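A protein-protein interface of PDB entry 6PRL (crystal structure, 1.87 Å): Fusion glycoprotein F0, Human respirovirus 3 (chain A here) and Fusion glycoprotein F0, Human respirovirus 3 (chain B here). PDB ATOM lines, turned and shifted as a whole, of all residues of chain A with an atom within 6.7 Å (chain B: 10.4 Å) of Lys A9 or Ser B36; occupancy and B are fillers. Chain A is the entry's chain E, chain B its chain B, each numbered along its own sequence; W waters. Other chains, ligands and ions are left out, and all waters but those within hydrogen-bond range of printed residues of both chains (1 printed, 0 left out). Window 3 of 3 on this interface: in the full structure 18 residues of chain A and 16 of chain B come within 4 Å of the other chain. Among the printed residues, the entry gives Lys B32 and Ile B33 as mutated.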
ATOM      1  N   ARG A   4       5.844 -12.170  24.750  1.00  0.00           N
ATOM      2  CA  ARG A   4       6.137 -10.817  24.298  1.00  0.00           C
ATOM      3  C   ARG A   4       5.835  -9.791  25.389  1.00  0.00           C
ATOM      4  O   ARG A   4       6.188  -8.620  25.263  1.00  0.00           O
ATOM      5  CB  ARG A   4       5.334 -10.488  23.037  1.00  0.00           C
ATOM      6  N   SER A   5       5.177 -10.234  26.456  1.00  0.00           N
ATOM      7  CA  SER A   5       4.865  -9.339  27.560  1.00  0.00           C
ATOM      8  C   SER A   5       6.129  -9.018  28.348  1.00  0.00           C
ATOM      9  O   SER A   5       7.094  -9.788  28.359  1.00  0.00           O
ATOM     10  CB  SER A   5       3.823  -9.963  28.484  1.00  0.00           C
ATOM     11  OG  SER A   5       4.417 -10.912  29.347  1.00  0.00           O
ATOM     12  N   ASP A   6       6.116  -7.859  29.015  1.00  0.00           N
ATOM     13  CA  ASP A   6       7.276  -7.468  29.815  1.00  0.00           C
ATOM     14  C   ASP A   6       7.568  -8.486  30.909  1.00  0.00           C
ATOM     15  O   ASP A   6       8.738  -8.720  31.239  1.00  0.00           O
ATOM     16  CB  ASP A   6       7.048  -6.081  30.423  1.00  0.00           C
ATOM     17  CG  ASP A   6       7.066  -4.976  29.381  1.00  0.00           C
ATOM     18  OD1 ASP A   6       7.429  -5.258  28.218  1.00  0.00           O
ATOM     19  OD2 ASP A   6       6.715  -3.826  29.724  1.00  0.00           O
ATOM     20  N   ILE A   7       6.530  -9.101  31.477  1.00  0.00           N
ATOM     21  CA  ILE A   7       6.739 -10.148  32.470  1.00  0.00           C
ATOM     22  C   ILE A   7       7.437 -11.347  31.839  1.00  0.00           C
ATOM     23  O   ILE A   7       8.333 -11.954  32.443  1.00  0.00           O
ATOM     24  CB  ILE A   7       5.399 -10.544  33.124  1.00  0.00           C
ATOM     25  CG1 ILE A   7       4.981  -9.473  34.138  1.00  0.00           C
ATOM     26  CG2 ILE A   7       5.504 -11.918  33.775  1.00  0.00           C
ATOM     27  CD1 ILE A   7       3.734  -9.808  34.937  1.00  0.00           C
ATOM     28  N   GLU A   8       7.038 -11.715  30.618  1.00  0.00           N
ATOM     29  CA  GLU A   8       7.683 -12.836  29.943  1.00  0.00           C
ATOM     30  C   GLU A   8       9.140 -12.523  29.627  1.00  0.00           C
ATOM     31  O   GLU A   8      10.002 -13.410  29.705  1.00  0.00           O
ATOM     32  CB  GLU A   8       6.919 -13.193  28.665  1.00  0.00           C
ATOM     33  CG  GLU A   8       5.573 -13.858  28.908  1.00  0.00           C
ATOM     34  CD  GLU A   8       5.005 -14.507  27.655  1.00  0.00           C
ATOM     35  OE1 GLU A   8       5.171 -15.735  27.493  1.00  0.00           O
ATOM     36  OE2 GLU A   8       4.404 -13.788  26.831  1.00  0.00           O
ATOM     37  N   LYS A   9       9.441 -11.270  29.280  1.00  0.00           N
ATOM     38  CA  LYS A   9      10.816 -10.902  28.960  1.00  0.00           C
ATOM     39  C   LYS A   9      11.700 -10.962  30.200  1.00  0.00           C
ATOM     40  O   LYS A   9      12.803 -11.523  30.161  1.00  0.00           O
ATOM     41  CB  LYS A   9      10.853  -9.512  28.327  1.00  0.00           C
ATOM     42  CG  LYS A   9      10.209  -9.462  26.949  1.00  0.00           C
ATOM     43  CD  LYS A   9      10.327  -8.080  26.323  1.00  0.00           C
ATOM     44  CE  LYS A   9       9.707  -8.054  24.934  1.00  0.00           C
ATOM     45  NZ  LYS A   9       9.804  -6.709  24.299  1.00  0.00           N
ATOM     46  N   LEU A  10      11.234 -10.389  31.316  1.00  0.00           N
ATOM     47  CA  LEU A  10      11.985 -10.495  32.564  1.00  0.00           C
ATOM     48  C   LEU A  10      12.203 -11.953  32.943  1.00  0.00           C
ATOM     49  O   LEU A  10      13.283 -12.330  33.416  1.00  0.00           O
ATOM     50  CB  LEU A  10      11.249  -9.759  33.681  1.00  0.00           C
ATOM     51  CG  LEU A  10      11.079  -8.251  33.508  1.00  0.00           C
ATOM     52  CD1 LEU A  10      10.053  -7.712  34.503  1.00  0.00           C
ATOM     53  CD2 LEU A  10      12.410  -7.537  33.675  1.00  0.00           C
ATOM     54  N   LYS A  11      11.187 -12.794  32.735  1.00  0.00           N
ATOM     55  CA  LYS A  11      11.314 -14.214  33.043  1.00  0.00           C
ATOM     56  C   LYS A  11      12.434 -14.848  32.228  1.00  0.00           C
ATOM     57  O   LYS A  11      13.267 -15.595  32.765  1.00  0.00           O
ATOM     58  CB  LYS A  11       9.976 -14.912  32.781  1.00  0.00           C
ATOM     59  CG  LYS A  11       9.987 -16.414  32.979  1.00  0.00           C
ATOM     60  CD  LYS A  11       8.588 -16.993  32.800  1.00  0.00           C
ATOM     61  CE  LYS A  11       8.613 -18.512  32.761  1.00  0.00           C
ATOM     62  NZ  LYS A  11       7.241 -19.098  32.758  1.00  0.00           N
ATOM     63  N   GLU A  12      12.485 -14.548  30.927  1.00  0.00           N
ATOM     64  CA  GLU A  12      13.530 -15.116  30.081  1.00  0.00           C
ATOM     65  C   GLU A  12      14.898 -14.542  30.429  1.00  0.00           C
ATOM     66  O   GLU A  12      15.914 -15.250  30.359  1.00  0.00           O
ATOM     67  CB  GLU A  12      13.212 -14.867  28.608  1.00  0.00           C
ATOM     68  CG  GLU A  12      12.018 -15.647  28.081  1.00  0.00           C
ATOM     69  CD  GLU A  12      12.157 -17.143  28.293  1.00  0.00           C
ATOM     70  OE1 GLU A  12      11.381 -17.705  29.093  1.00  0.00           O
ATOM     71  OE2 GLU A  12      13.051 -17.753  27.670  1.00  0.00           O
ATOM     72  N   ALA A  13      14.952 -13.259  30.789  1.00  0.00           N
ATOM     73  CA  ALA A  13      16.223 -12.659  31.186  1.00  0.00           C
ATOM     74  C   ALA A  13      16.816 -13.390  32.384  1.00  0.00           C
ATOM     75  O   ALA A  13      18.013 -13.712  32.402  1.00  0.00           O
ATOM     76  CB  ALA A  13      16.023 -11.175  31.497  1.00  0.00           C
ATOM     77  N   ILE A  14      15.989 -13.669  33.396  1.00  0.00           N
ATOM     78  CA  ILE A  14      16.470 -14.386  34.571  1.00  0.00           C
ATOM     79  C   ILE A  14      16.910 -15.791  34.185  1.00  0.00           C
ATOM     80  O   ILE A  14      17.913 -16.305  34.691  1.00  0.00           O
ATOM     81  CB  ILE A  14      15.390 -14.421  35.666  1.00  0.00           C
ATOM     82  CG1 ILE A  14      14.961 -13.007  36.043  1.00  0.00           C
ATOM     83  CG2 ILE A  14      15.912 -15.157  36.901  1.00  0.00           C
ATOM     84  CD1 ILE A  14      13.710 -12.960  36.903  1.00  0.00           C
ATOM     85  N   ARG B  28      25.130 -11.905  27.875  1.00  0.00           N
ATOM     86  CA  ARG B  28      24.839 -11.070  26.715  1.00  0.00           C
ATOM     87  C   ARG B  28      23.395 -11.254  26.266  1.00  0.00           C
ATOM     88  O   ARG B  28      22.690 -10.273  25.989  1.00  0.00           O
ATOM     89  CB  ARG B  28      25.804 -11.400  25.577  1.00  0.00           C
ATOM     90  CG  ARG B  28      25.856 -10.345  24.487  1.00  0.00           C
ATOM     91  CD  ARG B  28      26.435 -10.899  23.195  1.00  0.00           C
ATOM     92  NE  ARG B  28      25.601 -11.963  22.642  1.00  0.00           N
ATOM     93  CZ  ARG B  28      24.479 -11.759  21.957  1.00  0.00           C
ATOM     94  NH1 ARG B  28      24.044 -10.526  21.736  1.00  0.00           N
ATOM     95  NH2 ARG B  28      23.789 -12.792  21.496  1.00  0.00           N
ATOM     96  N   ARG B  29      22.930 -12.503  26.197  1.00  0.00           N
ATOM     97  CA  ARG B  29      21.544 -12.751  25.817  1.00  0.00           C
ATOM     98  C   ARG B  29      20.582 -12.144  26.832  1.00  0.00           C
ATOM     99  O   ARG B  29      19.515 -11.637  26.463  1.00  0.00           O
ATOM    100  CB  ARG B  29      21.292 -14.253  25.683  1.00  0.00           C
ATOM    101  CG  ARG B  29      22.030 -14.930  24.539  1.00  0.00           C
ATOM    102  CD  ARG B  29      21.507 -16.350  24.330  1.00  0.00           C
ATOM    103  NE  ARG B  29      22.209 -17.062  23.264  1.00  0.00           N
ATOM    104  CZ  ARG B  29      23.178 -17.956  23.457  1.00  0.00           C
ATOM    105  NH1 ARG B  29      23.745 -18.545  22.414  1.00  0.00           N
ATOM    106  NH2 ARG B  29      23.582 -18.268  24.682  1.00  0.00           N
ATOM    107  N   SER B  30      20.937 -12.192  28.116  1.00  0.00           N
ATOM    108  CA  SER B  30      20.060 -11.657  29.151  1.00  0.00           C
ATOM    109  C   SER B  30      19.925 -10.145  29.025  1.00  0.00           C
ATOM    110  O   SER B  30      18.812  -9.606  29.065  1.00  0.00           O
ATOM    111  CB  SER B  30      20.589 -12.036  30.534  1.00  0.00           C
ATOM    112  OG  SER B  30      19.801 -11.458  31.560  1.00  0.00           O
ATOM    113  N   ASN B  31      21.049  -9.438  28.886  1.00  0.00           N
ATOM    114  CA  ASN B  31      20.984  -7.990  28.713  1.00  0.00           C
ATOM    115  C   ASN B  31      20.266  -7.624  27.421  1.00  0.00           C
ATOM    116  O   ASN B  31      19.542  -6.622  27.366  1.00  0.00           O
ATOM    117  CB  ASN B  31      22.390  -7.397  28.732  1.00  0.00           C
ATOM    118  CG  ASN B  31      23.019  -7.452  30.103  1.00  0.00           C
ATOM    119  OD1 ASN B  31      22.321  -7.444  31.117  1.00  0.00           O
ATOM    120  ND2 ASN B  31      24.342  -7.503  30.145  1.00  0.00           N
ATOM    121  N   LYS B  32      20.449  -8.426  26.371  1.00  0.00           N
ATOM    122  CA  LYS B  32      19.752  -8.174  25.115  1.00  0.00           C
ATOM    123  C   LYS B  32      18.243  -8.232  25.303  1.00  0.00           C
ATOM    124  O   LYS B  32      17.503  -7.448  24.696  1.00  0.00           O
ATOM    125  CB  LYS B  32      20.207  -9.182  24.060  1.00  0.00           C
ATOM    126  CG  LYS B  32      19.544  -9.020  22.702  1.00  0.00           C
ATOM    127  CD  LYS B  32      20.120  -9.995  21.677  1.00  0.00           C
ATOM    128  CE  LYS B  32      19.903 -11.447  22.089  1.00  0.00           C
ATOM    129  NZ  LYS B  32      20.441 -12.402  21.079  1.00  0.00           N
ATOM    130  N   ILE B  33      17.765  -9.151  26.144  1.00  0.00           N
ATOM    131  CA  ILE B  33      16.333  -9.243  26.408  1.00  0.00           C
ATOM    132  C   ILE B  33      15.859  -8.034  27.204  1.00  0.00           C
ATOM    133  O   ILE B  33      14.804  -7.451  26.910  1.00  0.00           O
ATOM    134  CB  ILE B  33      16.008 -10.562  27.137  1.00  0.00           C
ATOM    135  CG1 ILE B  33      16.217 -11.751  26.196  1.00  0.00           C
ATOM    136  CG2 ILE B  33      14.587 -10.536  27.676  1.00  0.00           C
ATOM    137  CD1 ILE B  33      16.133 -13.105  26.878  1.00  0.00           C
ATOM    138  N   LEU B  34      16.620  -7.641  28.230  1.00  0.00           N
ATOM    139  CA  LEU B  34      16.246  -6.477  29.024  1.00  0.00           C
ATOM    140  C   LEU B  34      16.234  -5.210  28.182  1.00  0.00           C
ATOM    141  O   LEU B  34      15.468  -4.280  28.470  1.00  0.00           O
ATOM    142  CB  LEU B  34      17.202  -6.322  30.205  1.00  0.00           C
ATOM    143  CG  LEU B  34      17.230  -7.473  31.211  1.00  0.00           C
ATOM    144  CD1 LEU B  34      18.414  -7.329  32.161  1.00  0.00           C
ATOM    145  CD2 LEU B  34      15.930  -7.544  31.989  1.00  0.00           C
ATOM    146  N   ASP B  35      17.065  -5.151  27.136  1.00  0.00           N
ATOM    147  CA  ASP B  35      17.072  -3.980  26.267  1.00  0.00           C
ATOM    148  C   ASP B  35      15.758  -3.830  25.509  1.00  0.00           C
ATOM    149  O   ASP B  35      15.378  -2.711  25.145  1.00  0.00           O
ATOM    150  CB  ASP B  35      18.238  -4.063  25.283  1.00  0.00           C
ATOM    151  CG  ASP B  35      19.580  -3.821  25.947  1.00  0.00           C
ATOM    152  OD1 ASP B  35      19.602  -3.478  27.150  1.00  0.00           O
ATOM    153  OD2 ASP B  35      20.614  -3.972  25.265  1.00  0.00           O
ATOM    154  N   SER B  36      15.054  -4.931  25.259  1.00  0.00           N
ATOM    155  CA  SER B  36      13.777  -4.873  24.555  1.00  0.00           C
ATOM    156  C   SER B  36      12.618  -4.495  25.468  1.00  0.00           C
ATOM    157  O   SER B  36      11.456  -4.629  25.059  1.00  0.00           O
ATOM    158  CB  SER B  36      13.486  -6.216  23.879  1.00  0.00           C
ATOM    159  OG  SER B  36      13.219  -7.229  24.833  1.00  0.00           O
ATOM    160  N   ILE B  37      12.901  -4.027  26.680  1.00  0.00           N
ATOM    161  CA  ILE B  37      11.859  -3.612  27.612  1.00  0.00           C
ATOM    162  C   ILE B  37      11.763  -2.090  27.631  1.00  0.00           C
ATOM    163  O   ILE B  37      11.172  -1.484  26.737  1.00  0.00           O
ATOM    164  CB  ILE B  37      12.122  -4.164  29.027  1.00  0.00           C
ATOM    165  CG1 ILE B  37      12.006  -5.692  29.022  1.00  0.00           C
ATOM    166  CG2 ILE B  37      11.155  -3.545  30.029  1.00  0.00           C
ATOM    167  CD1 ILE B  37      12.409  -6.351  30.323  1.00  0.00           C
HETATM  168  O   HOH W   1       8.617  -2.933  26.588  1.00  0.00           O
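Lys A9 touches just these residues of chain B: Ile B33, Ser B36 and Ile B37. Ser B36 touches one residue of chain A. No residue of chain B comes within 4 Å of Ser A5. Of chain B, only Leu B34 (3.9 Å) and Ile B37 (3.6 Å) come within 4 Å of Leu A10. Of chain B, only Ser B30 and Leu B34 come within 4 Å of Ala A13. Of the printed residues of chain A, Ile B33 touches Lys A9 (3.2 Å) and Glu A12 (3.8 Å). Printed residues of chain A within 4 Å of Leu B34: Leu A10 and Ala A13. Printed residues of chain A within 4 Å of Ile B37: Lys A9 and Leu A10.
Among the printed residues, merely in contact across the chains: Lys A9 with Ile B33, Lys A9 with Ile B37, Leu A10 with Leu B34, Leu A10 with Ile B37, Glu A12 with Ile B33 and Ala A13 with Leu B34.
The backbone carbonyl oxygen (O) of Ser B36 sits at hydrogen-bond distance from the side-chain amino group (NZ) of Lys A9 (2.8 Å). The backbone carbonyl oxygen of Ala A13 is in hydrogen-bond range of the side-chain hydroxyl of Ser B30 (3.0 Å).
O of Ile B33 lies within hydrogen-bond range of OG of Ser B36.
Water W1 lies within hydrogen-bond range of O of Ile B37 (2.9 Å) and OD1 of Asp A6 (3.1 Å).
Of the 11 printed residues of chain A, 4 touch a printed residue of chain B. Printed residues of chain A that touch a printed residue of chain B: Lys A9, Leu A10, Glu A12 and Ala A13. Of the 10 printed residues of chain B, 5 touch a printed residue of chain A. Printed residues of chain B that touch a printed residue of chain A: Ser B30, Ile B33, Leu B34, Ser B36 and Ile B37. Among the printed residues, 8 pairs touch across the chains. Among the printed residues, no Asp or Glu carboxylate lies within 4 Å of a Lys or Arg side-chain nitrogen of the other chain.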
